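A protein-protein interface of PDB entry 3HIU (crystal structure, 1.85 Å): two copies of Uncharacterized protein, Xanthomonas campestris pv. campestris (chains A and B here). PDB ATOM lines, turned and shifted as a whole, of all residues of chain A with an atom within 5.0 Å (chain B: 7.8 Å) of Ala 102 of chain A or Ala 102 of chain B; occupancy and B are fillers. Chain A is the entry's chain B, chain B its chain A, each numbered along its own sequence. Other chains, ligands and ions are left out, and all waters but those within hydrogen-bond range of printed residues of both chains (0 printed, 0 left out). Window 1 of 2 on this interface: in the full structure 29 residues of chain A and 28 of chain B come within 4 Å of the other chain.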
ATOM      1  N   GLY A  98      14.207   5.562  -9.209  1.00  0.00           N
ATOM      2  CA  GLY A  98      15.094   5.410  -8.070  1.00  0.00           C
ATOM      3  C   GLY A  98      15.063   4.017  -7.444  1.00  0.00           C
ATOM      4  O   GLY A  98      16.101   3.427  -7.133  1.00  0.00           O
ATOM      5  N   ILE A  99      13.866   3.482  -7.244  1.00  0.00           N
ATOM      6  CA  ILE A  99      13.751   2.131  -6.734  1.00  0.00           C
ATOM      7  C   ILE A  99      14.216   1.156  -7.816  1.00  0.00           C
ATOM      8  O   ILE A  99      14.839   0.142  -7.518  1.00  0.00           O
ATOM      9  CB  ILE A  99      12.299   1.802  -6.351  1.00  0.00           C
ATOM     10  CG1 ILE A  99      11.687   2.931  -5.523  1.00  0.00           C
ATOM     11  CG2 ILE A  99      12.233   0.495  -5.586  1.00  0.00           C
ATOM     12  CD1 ILE A  99      10.183   2.807  -5.363  1.00  0.00           C
ATOM     13  N   SER A 100      13.908   1.473  -9.074  1.00  0.00           N
ATOM     14  CA  SER A 100      14.303   0.628 -10.201  1.00  0.00           C
ATOM     15  C   SER A 100      15.788   0.410 -10.162  1.00  0.00           C
ATOM     16  O   SER A 100      16.281  -0.696 -10.379  1.00  0.00           O
ATOM     17  CB  SER A 100      13.966   1.292 -11.533  1.00  0.00           C
ATOM     18  OG  SER A 100      12.622   1.088 -11.891  1.00  0.00           O
ATOM     19  N   TYR A 101      16.498   1.496  -9.907  1.00  0.00           N
ATOM     20  CA  TYR A 101      17.955   1.492  -9.893  1.00  0.00           C
ATOM     21  C   TYR A 101      18.521   0.714  -8.688  1.00  0.00           C
ATOM     22  O   TYR A 101      19.484  -0.045  -8.834  1.00  0.00           O
ATOM     23  CB  TYR A 101      18.447   2.943  -9.914  1.00  0.00           C
ATOM     24  CG  TYR A 101      19.943   3.135  -9.810  1.00  0.00           C
ATOM     25  CD1 TYR A 101      20.768   3.004 -10.933  1.00  0.00           C
ATOM     26  CD2 TYR A 101      20.531   3.483  -8.594  1.00  0.00           C
ATOM     27  CE1 TYR A 101      22.140   3.200 -10.838  1.00  0.00           C
ATOM     28  CE2 TYR A 101      21.899   3.678  -8.490  1.00  0.00           C
ATOM     29  CZ  TYR A 101      22.701   3.534  -9.610  1.00  0.00           C
ATOM     30  OH  TYR A 101      24.064   3.728  -9.495  1.00  0.00           O
ATOM     31  N   ALA A 102      17.905   0.893  -7.514  1.00  0.00           N
ATOM     32  CA  ALA A 102      18.317   0.212  -6.283  1.00  0.00           C
ATOM     33  C   ALA A 102      18.083  -1.293  -6.342  1.00  0.00           C
ATOM     34  O   ALA A 102      18.914  -2.063  -5.880  1.00  0.00           O
ATOM     35  CB  ALA A 102      17.604   0.804  -5.075  1.00  0.00           C
ATOM     36  N   PHE A 103      16.950  -1.711  -6.902  1.00  0.00           N
ATOM     37  CA  PHE A 103      16.691  -3.138  -7.061  1.00  0.00           C
ATOM     38  C   PHE A 103      17.674  -3.759  -8.047  1.00  0.00           C
ATOM     39  O   PHE A 103      18.124  -4.883  -7.842  1.00  0.00           O
ATOM     40  CB  PHE A 103      15.245  -3.410  -7.495  1.00  0.00           C
ATOM     41  CG  PHE A 103      14.781  -4.837  -7.234  1.00  0.00           C
ATOM     42  CD1 PHE A 103      14.804  -5.793  -8.248  1.00  0.00           C
ATOM     43  CD2 PHE A 103      14.317  -5.221  -5.970  1.00  0.00           C
ATOM     44  CE1 PHE A 103      14.375  -7.105  -8.006  1.00  0.00           C
ATOM     45  CE2 PHE A 103      13.882  -6.525  -5.724  1.00  0.00           C
ATOM     46  CZ  PHE A 103      13.912  -7.464  -6.744  1.00  0.00           C
ATOM     47  N   GLU A 104      18.013  -3.030  -9.110  1.00  0.00           N
ATOM     48  CA  GLU A 104      18.975  -3.514 -10.107  1.00  0.00           C
ATOM     49  C   GLU A 104      20.358  -3.658  -9.475  1.00  0.00           C
ATOM     50  O   GLU A 104      21.229  -4.359 -10.002  1.00  0.00           O
ATOM     51  CB  GLU A 104      19.058  -2.574 -11.318  1.00  0.00           C
ATOM     52  CG  GLU A 104      17.797  -2.506 -12.191  1.00  0.00           C
ATOM     53  CD  GLU A 104      17.467  -3.828 -12.874  1.00  0.00           C
ATOM     54  OE1 GLU A 104      18.229  -4.802 -12.715  1.00  0.00           O
ATOM     55  OE2 GLU A 104      16.438  -3.890 -13.576  1.00  0.00           O
ATOM     56  N   HIS A 105      20.565  -2.978  -8.350  1.00  0.00           N
ATOM     57  CA  HIS A 105      21.798  -3.166  -7.597  1.00  0.00           C
ATOM     58  C   HIS A 105      21.680  -4.268  -6.535  1.00  0.00           C
ATOM     59  O   HIS A 105      22.645  -4.968  -6.247  1.00  0.00           O
ATOM     60  CB  HIS A 105      22.302  -1.833  -7.036  1.00  0.00           C
ATOM     61  CG  HIS A 105      23.150  -1.076  -8.008  1.00  0.00           C
ATOM     62  ND1 HIS A 105      22.640  -0.114  -8.861  1.00  0.00           N
ATOM     63  CD2 HIS A 105      24.474  -1.166  -8.299  1.00  0.00           C
ATOM     64  CE1 HIS A 105      23.613   0.361  -9.617  1.00  0.00           C
ATOM     65  NE2 HIS A 105      24.733  -0.256  -9.295  1.00  0.00           N
ATOM     66  N   LEU A 106      20.487  -4.435  -5.974  1.00  0.00           N
ATOM     67  CA  LEU A 106      20.207  -5.617  -5.184  1.00  0.00           C
ATOM     68  C   LEU A 106      20.538  -6.823  -6.040  1.00  0.00           C
ATOM     69  O   LEU A 106      21.248  -7.722  -5.617  1.00  0.00           O
ATOM     70  CB  LEU A 106      18.731  -5.660  -4.782  1.00  0.00           C
ATOM     71  CG  LEU A 106      18.349  -6.753  -3.780  1.00  0.00           C
ATOM     72  CD1 LEU A 106      19.308  -6.738  -2.604  1.00  0.00           C
ATOM     73  CD2 LEU A 106      16.907  -6.576  -3.300  1.00  0.00           C
ATOM     74  N   LYS B  95      23.865 -11.390   2.687  1.00  0.00           N
ATOM     75  CA  LYS B  95      22.588 -10.847   2.241  1.00  0.00           C
ATOM     76  C   LYS B  95      22.399  -9.413   2.719  1.00  0.00           C
ATOM     77  O   LYS B  95      21.866  -8.572   1.995  1.00  0.00           O
ATOM     78  CB  LYS B  95      21.437 -11.724   2.736  1.00  0.00           C
ATOM     79  CG  LYS B  95      21.456 -13.140   2.176  1.00  0.00           C
ATOM     80  CD  LYS B  95      21.222 -13.161   0.673  1.00  0.00           C
ATOM     81  CE  LYS B  95      21.123 -14.588   0.137  1.00  0.00           C
ATOM     82  NZ  LYS B  95      20.923 -14.634  -1.342  1.00  0.00           N
ATOM     83  N   GLY B  96      22.832  -9.139   3.945  1.00  0.00           N
ATOM     84  CA  GLY B  96      22.739  -7.800   4.502  1.00  0.00           C
ATOM     85  C   GLY B  96      23.717  -6.878   3.805  1.00  0.00           C
ATOM     86  O   GLY B  96      23.458  -5.679   3.629  1.00  0.00           O
ATOM     87  N   VAL B  97      24.853  -7.439   3.399  1.00  0.00           N
ATOM     88  CA  VAL B  97      25.803  -6.687   2.595  1.00  0.00           C
ATOM     89  C   VAL B  97      25.160  -6.289   1.271  1.00  0.00           C
ATOM     90  O   VAL B  97      25.394  -5.191   0.767  1.00  0.00           O
ATOM     91  CB  VAL B  97      27.100  -7.473   2.351  1.00  0.00           C
ATOM     92  CG1 VAL B  97      27.978  -6.725   1.356  1.00  0.00           C
ATOM     93  CG2 VAL B  97      27.843  -7.687   3.663  1.00  0.00           C
ATOM     94  N   GLY B  98      24.331  -7.176   0.724  1.00  0.00           N
ATOM     95  CA  GLY B  98      23.651  -6.916  -0.528  1.00  0.00           C
ATOM     96  C   GLY B  98      22.546  -5.876  -0.424  1.00  0.00           C
ATOM     97  O   GLY B  98      22.338  -5.054  -1.326  1.00  0.00           O
ATOM     98  N   ILE B  99      21.820  -5.912   0.678  1.00  0.00           N
ATOM     99  CA  ILE B  99      20.790  -4.915   0.932  1.00  0.00           C
ATOM    100  C   ILE B  99      21.407  -3.560   1.276  1.00  0.00           C
ATOM    101  O   ILE B  99      20.831  -2.510   1.001  1.00  0.00           O
ATOM    102  CB  ILE B  99      19.894  -5.357   2.092  1.00  0.00           C
ATOM    103  CG1 ILE B  99      19.146  -6.637   1.716  1.00  0.00           C
ATOM    104  CG2 ILE B  99      18.939  -4.236   2.497  1.00  0.00           C
ATOM    105  CD1 ILE B  99      18.783  -7.477   2.925  1.00  0.00           C
ATOM    106  N   SER B 100      22.582  -3.591   1.891  1.00  0.00           N
ATOM    107  CA  SER B 100      23.291  -2.367   2.230  1.00  0.00           C
ATOM    108  C   SER B 100      23.645  -1.639   0.956  1.00  0.00           C
ATOM    109  O   SER B 100      23.480  -0.424   0.840  1.00  0.00           O
ATOM    110  CB  SER B 100      24.582  -2.693   2.976  1.00  0.00           C
ATOM    111  OG  SER B 100      24.304  -3.185   4.263  1.00  0.00           O
ATOM    112  N   TYR B 101      24.154  -2.409   0.007  1.00  0.00           N
ATOM    113  CA  TYR B 101      24.585  -1.881  -1.274  1.00  0.00           C
ATOM    114  C   TYR B 101      23.397  -1.367  -2.115  1.00  0.00           C
ATOM    115  O   TYR B 101      23.509  -0.353  -2.810  1.00  0.00           O
ATOM    116  CB  TYR B 101      25.374  -2.968  -2.011  1.00  0.00           C
ATOM    117  CG  TYR B 101      25.859  -2.573  -3.378  1.00  0.00           C
ATOM    118  CD1 TYR B 101      27.067  -1.900  -3.543  1.00  0.00           C
ATOM    119  CD2 TYR B 101      25.113  -2.887  -4.513  1.00  0.00           C
ATOM    120  CE1 TYR B 101      27.507  -1.538  -4.800  1.00  0.00           C
ATOM    121  CE2 TYR B 101      25.547  -2.530  -5.772  1.00  0.00           C
ATOM    122  CZ  TYR B 101      26.741  -1.854  -5.912  1.00  0.00           C
ATOM    123  OH  TYR B 101      27.168  -1.501  -7.174  1.00  0.00           O
ATOM    124  N   ALA B 102      22.262  -2.059  -2.036  1.00  0.00           N
ATOM    125  CA  ALA B 102      21.048  -1.640  -2.730  1.00  0.00           C
ATOM    126  C   ALA B 102      20.456  -0.351  -2.150  1.00  0.00           C
ATOM    127  O   ALA B 102      19.944   0.504  -2.882  1.00  0.00           O
ATOM    128  CB  ALA B 102      20.020  -2.755  -2.684  1.00  0.00           C
ATOM    129  N   PHE B 103      20.505  -0.215  -0.830  1.00  0.00           N
ATOM    130  CA  PHE B 103      19.950   0.970  -0.188  1.00  0.00           C
ATOM    131  C   PHE B 103      20.826   2.184  -0.462  1.00  0.00           C
ATOM    132  O   PHE B 103      20.334   3.235  -0.855  1.00  0.00           O
ATOM    133  CB  PHE B 103      19.788   0.754   1.318  1.00  0.00           C
ATOM    134  CG  PHE B 103      19.023   1.854   2.009  1.00  0.00           C
ATOM    135  CD1 PHE B 103      17.632   1.856   2.014  1.00  0.00           C
ATOM    136  CD2 PHE B 103      19.694   2.887   2.651  1.00  0.00           C
ATOM    137  CE1 PHE B 103      16.925   2.874   2.650  1.00  0.00           C
ATOM    138  CE2 PHE B 103      18.994   3.905   3.285  1.00  0.00           C
ATOM    139  CZ  PHE B 103      17.607   3.894   3.287  1.00  0.00           C
ATOM    140  N   GLU B 104      22.128   2.035  -0.252  1.00  0.00           N
ATOM    141  CA  GLU B 104      23.072   3.100  -0.571  1.00  0.00           C
ATOM    142  C   GLU B 104      22.856   3.560  -2.007  1.00  0.00           C
ATOM    143  O   GLU B 104      23.083   4.720  -2.334  1.00  0.00           O
ATOM    144  CB  GLU B 104      24.523   2.646  -0.350  1.00  0.00           C
ATOM    145  CG  GLU B 104      24.930   2.508   1.129  1.00  0.00           C
ATOM    146  CD  GLU B 104      24.769   3.814   1.925  1.00  0.00           C
ATOM    147  OE1 GLU B 104      25.168   4.887   1.425  1.00  0.00           O
ATOM    148  OE2 GLU B 104      24.243   3.774   3.057  1.00  0.00           O
ATOM    149  N   HIS B 105      22.405   2.651  -2.867  1.00  0.00           N
ATOM    150  CA  HIS B 105      22.116   3.021  -4.250  1.00  0.00           C
ATOM    151  C   HIS B 105      20.752   3.693  -4.427  1.00  0.00           C
ATOM    152  O   HIS B 105      20.585   4.529  -5.304  1.00  0.00           O
ATOM    153  CB  HIS B 105      22.309   1.834  -5.196  1.00  0.00           C
ATOM    154  CG  HIS B 105      23.672   1.799  -5.809  1.00  0.00           C
ATOM    155  ND1 HIS B 105      24.699   1.030  -5.301  1.00  0.00           N
ATOM    156  CD2 HIS B 105      24.191   2.481  -6.856  1.00  0.00           C
ATOM    157  CE1 HIS B 105      25.784   1.219  -6.031  1.00  0.00           C
ATOM    158  NE2 HIS B 105      25.502   2.098  -6.978  1.00  0.00           N
ATOM    159  N   LEU B 106      19.801   3.326  -3.576  1.00  0.00           N
ATOM    160  CA  LEU B 106      18.559   4.054  -3.449  1.00  0.00           C
ATOM    161  C   LEU B 106      18.877   5.480  -3.029  1.00  0.00           C
ATOM    162  O   LEU B 106      18.360   6.447  -3.591  1.00  0.00           O
ATOM    163  CB  LEU B 106      17.690   3.390  -2.381  1.00  0.00           C
ATOM    164  CG  LEU B 106      16.308   3.990  -2.110  1.00  0.00           C
ATOM    165  CD1 LEU B 106      15.553   4.234  -3.400  1.00  0.00           C
ATOM    166  CD2 LEU B 106      15.537   3.047  -1.185  1.00  0.00           C
ATOM    167  N   GLU B 107      19.744   5.610  -2.035  1.00  0.00           N
ATOM    168  CA  GLU B 107      20.140   6.926  -1.543  1.00  0.00           C
ATOM    169  C   GLU B 107      20.755   7.788  -2.641  1.00  0.00           C
ATOM    170  O   GLU B 107      20.311   8.910  -2.887  1.00  0.00           O
ATOM    171  CB  GLU B 107      21.117   6.789  -0.373  1.00  0.00           C
ATOM    172  CG  GLU B 107      20.488   6.252   0.890  1.00  0.00           C
ATOM    173  CD  GLU B 107      21.336   6.528   2.107  1.00  0.00           C
ATOM    174  OE1 GLU B 107      20.937   7.380   2.923  1.00  0.00           O
ATOM    175  OE2 GLU B 107      22.411   5.906   2.241  1.00  0.00           O
ATOM    176  N   ILE B 108      21.789   7.260  -3.285  1.00  0.00           N
ATOM    177  CA  ILE B 108      22.405   7.942  -4.413  1.00  0.00           C
ATOM    178  C   ILE B 108      21.313   8.573  -5.271  1.00  0.00           C
ATOM    179  O   ILE B 108      21.117   9.783  -5.239  1.00  0.00           O
ATOM    180  CB  ILE B 108      23.262   6.984  -5.266  1.00  0.00           C
ATOM    181  CG1 ILE B 108      24.507   6.535  -4.492  1.00  0.00           C
ATOM    182  CG2 ILE B 108      23.653   7.645  -6.576  1.00  0.00           C
ATOM    183  CD1 ILE B 108      25.146   5.259  -5.050  1.00  0.00           C
ATOM    184  N   ALA B 109      20.583   7.744  -6.007  1.00  0.00           N
ATOM    185  CA  ALA B 109      19.527   8.224  -6.888  1.00  0.00           C
ATOM    186  C   ALA B 109      18.737   9.379  -6.275  1.00  0.00           C
ATOM    187  O   ALA B 109      18.483  10.388  -6.943  1.00  0.00           O
ATOM    188  CB  ALA B 109      18.595   7.086  -7.267  1.00  0.00           C
ATOM    189  N   ALA B 141      28.846   2.739  -0.830  1.00  0.00           N
ATOM    190  CA  ALA B 141      28.493   1.666  -1.761  1.00  0.00           C
ATOM    191  C   ALA B 141      29.757   1.112  -2.438  1.00  0.00           C
ATOM    192  O   ALA B 141      29.861  -0.086  -2.726  1.00  0.00           O
ATOM    193  CB  ALA B 141      27.490   2.183  -2.807  1.00  0.00           C
ATOM    194  N   LEU B 144      31.499  -1.261   0.043  1.00  0.00           N
ATOM    195  CA  LEU B 144      30.835  -2.551   0.146  1.00  0.00           C
ATOM    196  C   LEU B 144      31.111  -3.485  -1.036  1.00  0.00           C
ATOM    197  O   LEU B 144      31.427  -4.659  -0.844  1.00  0.00           O
ATOM    198  CB  LEU B 144      29.330  -2.375   0.311  1.00  0.00           C
ATOM    199  CG  LEU B 144      28.778  -1.766   1.595  1.00  0.00           C
ATOM    200  CD1 LEU B 144      27.305  -1.437   1.384  1.00  0.00           C
ATOM    201  CD2 LEU B 144      28.964  -2.720   2.749  1.00  0.00           C
ATOM    202  N   ILE B 145      30.978  -2.982  -2.257  1.00  0.00           N
ATOM    203  CA  ILE B 145      31.042  -3.866  -3.424  1.00  0.00           C
ATOM    204  C   ILE B 145      32.477  -4.300  -3.729  1.00  0.00           C
ATOM    205  O   ILE B 145      32.706  -5.345  -4.352  1.00  0.00           O
ATOM    206  CB  ILE B 145      30.369  -3.233  -4.665  1.00  0.00           C
ATOM    207  CG1 ILE B 145      29.888  -4.321  -5.639  1.00  0.00           C
ATOM    208  CG2 ILE B 145      31.295  -2.203  -5.317  1.00  0.00           C
ATOM    209  CD1 ILE B 145      28.622  -5.057  -5.192  1.00  0.00           C
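Among the printed residues, pairs that only touch across the chains: Gly 98 of chain A with Leu 106 of chain B (3.9 Å), Gly 98 of chain A with Ala 109 of chain B (3.96 Å), Ala 102 of chain A with Ala 102 of chain B (3.2 Å), Ala 102 of chain A with Leu 106 of chain B (3.7 Å), Leu 106 of chain A with Gly 98 of chain B (3.7 Å) and Leu 106 of chain A with Ala 102 of chain B (3.7 Å).
Gly 98 of chain A touches Leu 106 of chain B, and with the chains exchanged Leu 106 of chain A touches Gly 98 of chain B. Tyr 101 of chain A touches His 105 of chain B, and with the chains exchanged His 105 of chain A touches Tyr 101 of chain B. Ala 102 of chain B touches its own counterpart, Ala 102 of chain A. His 105 of chain A touches its own counterpart, His 105 of chain B. Of the 9 pairs that touch across the chains among the printed residues, 8 have their exchanged pair printed and touching as well.
Of chain B, only Ala 102 (3.2 Å) and Leu 106 (3.7 Å) come within 4 Å of Ala 102 of chain A. Ala 102 of chain B touches just these residues of chain A: Ala 102 (3.2 Å) and Leu 106 (3.7 Å). Of the printed residues of chain B, His 105 of chain A touches Tyr 101 and His 105. Of the printed residues of chain B, Tyr 101 of chain A touches His 105 (2.9 Å). The nearest printed residue of chain A that does not touch Ala 109 of chain B is Tyr 101 of chain A (4.3 Å).
NE2 of His 105 of chain A lies close to OH of Tyr 101 of chain B, at 3.5 Å. NE2 of His 105 of chain B sits close to OH of Tyr 101 of chain A (3.3 Å). A ring nitrogen (NE2) of His 105 of chain B sits at hydrogen-bond distance from a ring nitrogen (NE2) of His 105 of chain A, 3.4 Å away.
A ring nitrogen (ND1) of His 105 of chain B is in hydrogen-bond range of the backbone carbonyl oxygen of Tyr 101 of chain B, 3.1 Å away. O of Tyr 101 of chain A is in hydrogen-bond range of ND1 of His 105 of chain A.
Of the 18 printed residues of chain B, 6 touch a printed residue of chain A. Among the printed residues, 9 pairs touch across the chains.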
